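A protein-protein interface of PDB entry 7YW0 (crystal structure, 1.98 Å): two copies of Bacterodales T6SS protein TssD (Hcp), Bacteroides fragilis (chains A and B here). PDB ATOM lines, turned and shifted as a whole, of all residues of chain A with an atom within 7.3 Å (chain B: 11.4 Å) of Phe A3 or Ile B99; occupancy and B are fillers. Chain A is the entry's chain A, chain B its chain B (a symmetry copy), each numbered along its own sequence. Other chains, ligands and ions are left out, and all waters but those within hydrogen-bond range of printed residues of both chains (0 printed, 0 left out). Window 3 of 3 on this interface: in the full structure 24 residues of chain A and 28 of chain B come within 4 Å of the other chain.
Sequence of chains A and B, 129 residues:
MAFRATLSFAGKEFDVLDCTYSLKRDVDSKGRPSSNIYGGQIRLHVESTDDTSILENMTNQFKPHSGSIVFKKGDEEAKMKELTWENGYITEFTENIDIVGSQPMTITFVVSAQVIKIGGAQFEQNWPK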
ATOM      1  N   PHE A   3      10.439  20.392  -6.823  1.00  0.00           N
ATOM      2  CA  PHE A   3       9.096  20.681  -6.233  1.00  0.00           C
ATOM      3  C   PHE A   3       9.171  20.526  -4.716  1.00  0.00           C
ATOM      4  O   PHE A   3       8.742  21.408  -3.975  1.00  0.00           O
ATOM      5  CB  PHE A   3       8.013  19.809  -6.879  1.00  0.00           C
ATOM      6  CG  PHE A   3       7.309  20.455  -8.045  1.00  0.00           C
ATOM      7  CD1 PHE A   3       7.881  20.458  -9.315  1.00  0.00           C
ATOM      8  CD2 PHE A   3       6.077  21.074  -7.872  1.00  0.00           C
ATOM      9  CE1 PHE A   3       7.237  21.061 -10.387  1.00  0.00           C
ATOM     10  CE2 PHE A   3       5.433  21.672  -8.946  1.00  0.00           C
ATOM     11  CZ  PHE A   3       6.013  21.667 -10.198  1.00  0.00           C
ATOM     12  N   ARG A   4       9.725  19.394  -4.264  1.00  0.00           N
ATOM     13  CA  ARG A   4      10.151  19.224  -2.882  1.00  0.00           C
ATOM     14  C   ARG A   4      11.502  18.514  -2.856  1.00  0.00           C
ATOM     15  O   ARG A   4      11.711  17.543  -3.587  1.00  0.00           O
ATOM     16  CB  ARG A   4       9.096  18.473  -2.070  1.00  0.00           C
ATOM     17  CG  ARG A   4       9.153  18.754  -0.574  1.00  0.00           C
ATOM     18  CD  ARG A   4       9.571  20.189  -0.282  1.00  0.00           C
ATOM     19  NE  ARG A   4       8.667  20.880   0.629  1.00  0.00           N
ATOM     20  CZ  ARG A   4       7.930  21.943   0.316  1.00  0.00           C
ATOM     21  NH1 ARG A   4       7.133  22.482   1.222  1.00  0.00           N
ATOM     22  NH2 ARG A   4       7.997  22.469  -0.894  1.00  0.00           N
ATOM     23  N   ALA A   5      12.418  19.035  -2.031  1.00  0.00           N
ATOM     24  CA  ALA A   5      13.754  18.472  -1.926  1.00  0.00           C
ATOM     25  C   ALA A   5      14.148  18.310  -0.462  1.00  0.00           C
ATOM     26  O   ALA A   5      14.002  19.230   0.331  1.00  0.00           O
ATOM     27  CB  ALA A   5      14.741  19.322  -2.681  1.00  0.00           C
ATOM     28  N   ASP A  15      14.667  20.621   5.042  1.00  0.00           N
ATOM     29  CA  ASP A  15      13.918  20.943   3.844  1.00  0.00           C
ATOM     30  C   ASP A  15      14.779  21.857   2.966  1.00  0.00           C
ATOM     31  O   ASP A  15      15.338  22.849   3.428  1.00  0.00           O
ATOM     32  CB  ASP A  15      12.494  21.403   4.185  1.00  0.00           C
ATOM     33  CG  ASP A  15      11.690  21.760   2.951  1.00  0.00           C
ATOM     34  OD1 ASP A  15      11.433  20.845   2.128  1.00  0.00           O
ATOM     35  OD2 ASP A  15      11.370  22.957   2.800  1.00  0.00           O
ATOM     36  N   VAL A  16      14.911  21.499   1.686  1.00  0.00           N
ATOM     37  CA  VAL A  16      15.856  22.231   0.868  1.00  0.00           C
ATOM     38  C   VAL A  16      15.134  23.396   0.202  1.00  0.00           C
ATOM     39  O   VAL A  16      14.226  23.158  -0.565  1.00  0.00           O
ATOM     40  CB  VAL A  16      16.516  21.304  -0.169  1.00  0.00           C
ATOM     41  CG1 VAL A  16      17.087  22.100  -1.341  1.00  0.00           C
ATOM     42  CG2 VAL A  16      17.576  20.438   0.492  1.00  0.00           C
ATOM     43  N   LEU A  17      15.594  24.642   0.428  1.00  0.00           N
ATOM     44  CA  LEU A  17      15.007  25.748  -0.312  1.00  0.00           C
ATOM     45  C   LEU A  17      15.578  25.754  -1.724  1.00  0.00           C
ATOM     46  O   LEU A  17      14.851  25.961  -2.692  1.00  0.00           O
ATOM     47  CB  LEU A  17      15.271  27.073   0.418  1.00  0.00           C
ATOM     48  CG  LEU A  17      14.743  27.130   1.853  1.00  0.00           C
ATOM     49  CD1 LEU A  17      15.292  28.355   2.591  1.00  0.00           C
ATOM     50  CD2 LEU A  17      13.212  27.156   1.870  1.00  0.00           C
ATOM     51  N   ASP A  18      16.902  25.569  -1.852  1.00  0.00           N
ATOM     52  CA  ASP A  18      17.470  25.526  -3.190  1.00  0.00           C
ATOM     53  C   ASP A  18      18.793  24.774  -3.138  1.00  0.00           C
ATOM     54  O   ASP A  18      19.417  24.741  -2.080  1.00  0.00           O
ATOM     55  CB  ASP A  18      17.476  26.902  -3.881  1.00  0.00           C
ATOM     56  CG  ASP A  18      18.249  27.983  -3.144  1.00  0.00           C
ATOM     57  OD1 ASP A  18      19.493  27.878  -3.104  1.00  0.00           O
ATOM     58  OD2 ASP A  18      17.598  28.908  -2.599  1.00  0.00           O
ATOM     59  N   CYS A  19      19.162  24.150  -4.265  1.00  0.00           N
ATOM     60  CA  CYS A  19      20.353  23.327  -4.381  1.00  0.00           C
ATOM     61  C   CYS A  19      20.954  23.502  -5.773  1.00  0.00           C
ATOM     62  O   CYS A  19      20.212  23.521  -6.756  1.00  0.00           O
ATOM     63  CB  CYS A  19      19.941  21.858  -4.215  1.00  0.00           C
ATOM     64  SG  CYS A  19      21.328  20.722  -4.496  1.00  0.00           S
ATOM     65  N   PHE A  71      14.728  14.463  -4.543  1.00  0.00           N
ATOM     66  CA  PHE A  71      13.829  15.386  -5.221  1.00  0.00           C
ATOM     67  C   PHE A  71      12.520  14.682  -5.553  1.00  0.00           C
ATOM     68  O   PHE A  71      12.530  13.578  -6.085  1.00  0.00           O
ATOM     69  CB  PHE A  71      14.467  15.873  -6.514  1.00  0.00           C
ATOM     70  CG  PHE A  71      15.845  16.447  -6.338  1.00  0.00           C
ATOM     71  CD1 PHE A  71      16.007  17.766  -5.964  1.00  0.00           C
ATOM     72  CD2 PHE A  71      16.974  15.676  -6.551  1.00  0.00           C
ATOM     73  CE1 PHE A  71      17.273  18.315  -5.829  1.00  0.00           C
ATOM     74  CE2 PHE A  71      18.237  16.236  -6.431  1.00  0.00           C
ATOM     75  CZ  PHE A  71      18.384  17.545  -6.054  1.00  0.00           C
ATOM     76  N   LYS A  72      11.404  15.351  -5.253  1.00  0.00           N
ATOM     77  CA  LYS A  72      10.076  14.775  -5.404  1.00  0.00           C
ATOM     78  C   LYS A  72       9.204  15.689  -6.274  1.00  0.00           C
ATOM     79  O   LYS A  72       9.578  16.829  -6.547  1.00  0.00           O
ATOM     80  CB  LYS A  72       9.481  14.524  -4.016  1.00  0.00           C
ATOM     81  CG  LYS A  72       8.215  13.679  -3.986  1.00  0.00           C
ATOM     82  CD  LYS A  72       8.006  12.928  -2.689  1.00  0.00           C
ATOM     83  CE  LYS A  72       6.552  12.613  -2.398  1.00  0.00           C
ATOM     84  NZ  LYS A  72       5.803  13.809  -1.946  1.00  0.00           N
ATOM     85  N   LYS A  73       8.060  15.167  -6.744  1.00  0.00           N
ATOM     86  CA  LYS A  73       7.069  15.955  -7.467  1.00  0.00           C
ATOM     87  C   LYS A  73       5.671  15.600  -6.957  1.00  0.00           C
ATOM     88  O   LYS A  73       5.228  14.459  -7.085  1.00  0.00           O
ATOM     89  CB  LYS A  73       7.199  15.745  -8.980  1.00  0.00           C
ATOM     90  N   GLY A  74       4.998  16.589  -6.350  1.00  0.00           N
ATOM     91  CA  GLY A  74       3.709  16.397  -5.704  1.00  0.00           C
ATOM     92  C   GLY A  74       3.851  15.680  -4.371  1.00  0.00           C
ATOM     93  O   GLY A  74       4.130  14.459  -4.396  1.00  0.00           O
ATOM     94  N   MET A  80      11.709  11.405  -7.688  1.00  0.00           N
ATOM     95  CA  MET A  80      12.043  11.732  -9.065  1.00  0.00           C
ATOM     96  C   MET A  80      13.495  11.342  -9.367  1.00  0.00           C
ATOM     97  O   MET A  80      13.775  10.745 -10.409  1.00  0.00           O
ATOM     98  CB  MET A  80      11.806  13.222  -9.322  1.00  0.00           C
ATOM     99  CG  MET A  80      12.203  13.695 -10.702  1.00  0.00           C
ATOM    100  SD  MET A  80      12.179  15.501 -10.697  1.00  0.00           S
ATOM    101  CE  MET A  80      11.360  15.820 -12.258  1.00  0.00           C
ATOM    102  N   GLN A 103      12.945  34.852   2.861  1.00  0.00           N
ATOM    103  CA  GLN A 103      13.077  33.748   3.855  1.00  0.00           C
ATOM    104  C   GLN A 103      13.864  34.270   5.053  1.00  0.00           C
ATOM    105  O   GLN A 103      15.039  34.615   4.916  1.00  0.00           O
ATOM    106  CB  GLN A 103      13.726  32.518   3.212  1.00  0.00           C
ATOM    107  CG  GLN A 103      14.871  32.872   2.264  1.00  0.00           C
ATOM    108  CD  GLN A 103      14.725  32.310   0.867  1.00  0.00           C
ATOM    109  OE1 GLN A 103      13.805  31.547   0.567  1.00  0.00           O
ATOM    110  NE2 GLN A 103      15.647  32.685  -0.006  1.00  0.00           N
ATOM    111  N   GLU B  47      14.409  21.819 -18.996  1.00  0.00           N
ATOM    112  CA  GLU B  47      13.832  21.404 -17.728  1.00  0.00           C
ATOM    113  C   GLU B  47      14.478  20.101 -17.282  1.00  0.00           C
ATOM    114  O   GLU B  47      14.814  19.261 -18.114  1.00  0.00           O
ATOM    115  CB  GLU B  47      12.343  21.078 -17.847  1.00  0.00           C
ATOM    116  CG  GLU B  47      11.440  22.292 -17.823  1.00  0.00           C
ATOM    117  CD  GLU B  47      10.078  21.955 -18.409  1.00  0.00           C
ATOM    118  OE1 GLU B  47       9.287  21.316 -17.693  1.00  0.00           O
ATOM    119  OE2 GLU B  47       9.828  22.288 -19.601  1.00  0.00           O
ATOM    120  N   SER B  48      14.579  19.934 -15.959  1.00  0.00           N
ATOM    121  CA  SER B  48      14.997  18.681 -15.343  1.00  0.00           C
ATOM    122  C   SER B  48      13.817  17.719 -15.245  1.00  0.00           C
ATOM    123  O   SER B  48      12.696  18.130 -14.952  1.00  0.00           O
ATOM    124  CB  SER B  48      15.521  18.944 -13.967  1.00  0.00           C
ATOM    125  OG  SER B  48      16.642  19.798 -13.991  1.00  0.00           O
ATOM    126  N   THR B  49      14.064  16.428 -15.470  1.00  0.00           N
ATOM    127  CA  THR B  49      13.088  15.404 -15.102  1.00  0.00           C
ATOM    128  C   THR B  49      13.794  14.333 -14.273  1.00  0.00           C
ATOM    129  O   THR B  49      14.860  14.585 -13.721  1.00  0.00           O
ATOM    130  CB  THR B  49      12.402  14.780 -16.330  1.00  0.00           C
ATOM    131  OG1 THR B  49      13.406  14.012 -16.987  1.00  0.00           O
ATOM    132  CG2 THR B  49      11.793  15.782 -17.294  1.00  0.00           C
ATOM    133  N   ASP B  50      13.229  13.121 -14.247  1.00  0.00           N
ATOM    134  CA  ASP B  50      13.879  11.967 -13.643  1.00  0.00           C
ATOM    135  C   ASP B  50      15.152  11.597 -14.413  1.00  0.00           C
ATOM    136  O   ASP B  50      15.997  10.858 -13.915  1.00  0.00           O
ATOM    137  CB  ASP B  50      12.898  10.794 -13.547  1.00  0.00           C
ATOM    138  CG  ASP B  50      12.195  10.498 -14.859  1.00  0.00           C
ATOM    139  OD1 ASP B  50      11.884  11.452 -15.585  1.00  0.00           O
ATOM    140  OD2 ASP B  50      11.964   9.314 -15.140  1.00  0.00           O
ATOM    141  N   GLU B  95      23.042  22.027 -12.569  1.00  0.00           N
ATOM    142  CA  GLU B  95      21.617  21.770 -12.399  1.00  0.00           C
ATOM    143  C   GLU B  95      21.197  22.546 -11.165  1.00  0.00           C
ATOM    144  O   GLU B  95      21.959  22.572 -10.190  1.00  0.00           O
ATOM    145  CB  GLU B  95      21.382  20.267 -12.125  1.00  0.00           C
ATOM    146  CG  GLU B  95      19.908  19.850 -11.989  1.00  0.00           C
ATOM    147  CD  GLU B  95      19.574  18.380 -12.353  1.00  0.00           C
ATOM    148  OE1 GLU B  95      20.460  17.487 -12.207  1.00  0.00           O
ATOM    149  OE2 GLU B  95      18.404  18.094 -12.764  1.00  0.00           O
ATOM    150  N   ASN B  96      19.987  23.131 -11.191  1.00  0.00           N
ATOM    151  CA  ASN B  96      19.561  23.958 -10.065  1.00  0.00           C
ATOM    152  C   ASN B  96      18.119  23.608  -9.708  1.00  0.00           C
ATOM    153  O   ASN B  96      17.338  23.345 -10.607  1.00  0.00           O
ATOM    154  CB  ASN B  96      19.728  25.456 -10.370  1.00  0.00           C
ATOM    155  CG  ASN B  96      18.943  26.336  -9.409  1.00  0.00           C
ATOM    156  OD1 ASN B  96      19.379  26.618  -8.285  1.00  0.00           O
ATOM    157  ND2 ASN B  96      17.748  26.719  -9.829  1.00  0.00           N
ATOM    158  N   ILE B  97      17.819  23.531  -8.404  1.00  0.00           N
ATOM    159  CA  ILE B  97      16.475  23.332  -7.874  1.00  0.00           C
ATOM    160  C   ILE B  97      16.164  24.551  -7.020  1.00  0.00           C
ATOM    161  O   ILE B  97      17.038  25.022  -6.293  1.00  0.00           O
ATOM    162  CB  ILE B  97      16.452  22.049  -7.012  1.00  0.00           C
ATOM    163  CG1 ILE B  97      17.078  20.857  -7.737  1.00  0.00           C
ATOM    164  CG2 ILE B  97      15.050  21.729  -6.505  1.00  0.00           C
ATOM    165  CD1 ILE B  97      18.596  20.855  -7.802  1.00  0.00           C
ATOM    166  N   ASP B  98      14.984  25.076  -7.130  1.00  0.00           N
ATOM    167  CA  ASP B  98      14.648  26.249  -6.394  1.00  0.00           C
ATOM    168  C   ASP B  98      13.183  26.394  -6.245  1.00  0.00           C
ATOM    169  O   ASP B  98      12.548  26.844  -7.148  1.00  0.00           O
ATOM    170  CB  ASP B  98      15.114  27.446  -7.156  1.00  0.00           C
ATOM    171  CG  ASP B  98      15.034  28.677  -6.366  1.00  0.00           C
ATOM    172  OD1 ASP B  98      14.242  28.727  -5.431  1.00  0.00           O
ATOM    173  OD2 ASP B  98      15.775  29.612  -6.662  1.00  0.00           O
ATOM    174  N   ILE B  99      12.610  26.139  -5.096  1.00  0.00           N
ATOM    175  CA  ILE B  99      11.191  26.299  -4.974  1.00  0.00           C
ATOM    176  C   ILE B  99      10.720  27.757  -5.094  1.00  0.00           C
ATOM    177  O   ILE B  99      10.391  28.347  -4.082  1.00  0.00           O
ATOM    178  CB  ILE B  99      10.716  25.773  -3.653  1.00  0.00           C
ATOM    179  CG1 ILE B  99      11.021  24.308  -3.552  1.00  0.00           C
ATOM    180  CG2 ILE B  99       9.220  25.961  -3.605  1.00  0.00           C
ATOM    181  CD1 ILE B  99      12.465  24.017  -3.386  1.00  0.00           C
ATOM    182  N   VAL B 100      10.597  28.290  -6.324  1.00  0.00           N
ATOM    183  CA  VAL B 100      10.259  29.675  -6.601  1.00  0.00           C
ATOM    184  C   VAL B 100       9.888  29.833  -8.081  1.00  0.00           C
ATOM    185  O   VAL B 100      10.726  29.793  -9.003  1.00  0.00           O
ATOM    186  CB  VAL B 100      11.440  30.613  -6.271  1.00  0.00           C
ATOM    187  CG1 VAL B 100      11.562  31.705  -7.299  1.00  0.00           C
ATOM    188  CG2 VAL B 100      11.283  31.285  -4.922  1.00  0.00           C
ATOM    189  N   GLN B 103      11.345  28.920 -12.974  1.00  0.00           N
ATOM    190  CA  GLN B 103      11.352  27.492 -13.396  1.00  0.00           C
ATOM    191  C   GLN B 103      12.002  26.669 -12.287  1.00  0.00           C
ATOM    192  O   GLN B 103      13.174  26.874 -11.973  1.00  0.00           O
ATOM    193  CB  GLN B 103      12.048  27.338 -14.753  1.00  0.00           C
ATOM    194  N   PRO B 104      11.272  25.700 -11.680  1.00  0.00           N
ATOM    195  CA  PRO B 104      11.691  25.089 -10.416  1.00  0.00           C
ATOM    196  C   PRO B 104      13.010  24.321 -10.514  1.00  0.00           C
ATOM    197  O   PRO B 104      13.929  24.551  -9.730  1.00  0.00           O
ATOM    198  CB  PRO B 104      10.512  24.168 -10.052  1.00  0.00           C
ATOM    199  CG  PRO B 104       9.876  23.839 -11.386  1.00  0.00           C
ATOM    200  CD  PRO B 104      10.035  25.103 -12.209  1.00  0.00           C
ATOM    201  N   MET B 105      13.110  23.425 -11.495  1.00  0.00           N
ATOM    202  CA  MET B 105      14.266  22.551 -11.572  1.00  0.00           C
ATOM    203  C   MET B 105      14.765  22.486 -13.009  1.00  0.00           C
ATOM    204  O   MET B 105      14.010  22.100 -13.896  1.00  0.00           O
ATOM    205  CB  MET B 105      13.900  21.141 -11.099  1.00  0.00           C
ATOM    206  CG  MET B 105      15.134  20.288 -10.876  1.00  0.00           C
ATOM    207  SD  MET B 105      14.917  18.852  -9.793  1.00  0.00           S
ATOM    208  CE  MET B 105      16.556  18.128  -9.832  1.00  0.00           C
ATOM    209  N   THR B 106      16.046  22.839 -13.249  1.00  0.00           N
ATOM    210  CA  THR B 106      16.451  22.967 -14.636  1.00  0.00           C
ATOM    211  C   THR B 106      17.930  22.629 -14.732  1.00  0.00           C
ATOM    212  O   THR B 106      18.597  22.635 -13.713  1.00  0.00           O
ATOM    213  CB  THR B 106      16.270  24.396 -15.199  1.00  0.00           C
ATOM    214  OG1 THR B 106      17.266  25.273 -14.663  1.00  0.00           O
ATOM    215  CG2 THR B 106      14.883  24.977 -15.050  1.00  0.00           C
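O of Cys A19 sits at hydrogen-bond distance from N of Ile B97, at 2.9 Å.
N of Ile B99 sits close to O of Leu A17 (3.3 Å).
The side-chain hydroxyl of Thr B49 lies within hydrogen-bond range of the side-chain carboxylate of Asp B50 (3.3 Å).
N of Thr B106 sits at hydrogen-bond distance from OG of Ser B48, 3.2 Å away.
N of Val A16 sits at hydrogen-bond distance from O of Ala A5 (2.8 Å).
The backbone carbonyl oxygen of Met B105 lies within hydrogen-bond range of the backbone NH of Ser B48 (3.0 Å).
O of Pro B104 is in hydrogen-bond range of N of Asp B98, 2.9 Å away.
The backbone carbonyl oxygen (O) of Phe A71 sits at hydrogen-bond distance from the backbone NH (N) of Met A80 (2.8 Å).
Among the printed residues, merely in contact across the chains: Asp A18 with Ile B97, Phe A71 with Ile B97, Met A80 with Asp B50, Met A80 with Thr B49, Cys A19 with Asn B96, Val A16 with Ile B99, Phe A3 with Ile B99, Leu A17 with Asp B98, Met A80 with Ser B48, Asp A18 with Asp B98, Phe A71 with Met B105, Phe A3 with Pro B104 and Cys A19 with Glu B95.
Arg A4 touches none of the printed residues of chain B.
Val A16 touches one residue of chain B.
Printed residues of chain B within 4 Å of Asp A18: Ile B97 (3.1 Å) and Asp B98 (3.8 Å).
Of the printed residues of chain B, Cys A19 touches Glu B95, Asn B96 and Ile B97.
Printed residues of chain B within 4 Å of Phe A71: Ile B97 (3.2 Å) and Met B105 (3.9 Å).
Lys A72 touches none of the printed residues of chain B.
No residue of chain B comes within 4 Å of Lys A73.
No residue of chain B comes within 4 Å of Gly A74.
Of the printed residues of chain B, Met A80 touches Ser B48 (3.8 Å), Thr B49 (3.4 Å) and Asp B50 (3.3 Å).
Gln A103 touches none of the printed residues of chain B.
Of the printed residues of chain A, Ser B48 touches Met A80.
Ile B99 touches just these residues of chain A: Phe A3, Val A16 and Leu A17.
The nearest residue of chain A that does not touch Ile B99 is Arg A4 (4.4 Å).
The nearest printed residue of chain A that does not touch Ile B97 is Leu A17 (4.3 Å).
Hydrophobic or aromatic side chains of chain A that line the printed part of chain B: Phe A3, Phe A71 and Met A80.
Among the printed residues, 15 pairs touch across the chains.
Among the printed residues, no Asp or Glu carboxylate lies within 4 Å of a Lys or Arg side-chain nitrogen of the other chain.
Position printed for both chains: 103.
Of the 15 pairs that touch across the chains among the printed residues, none has its exchanged pair printed and touching as well.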
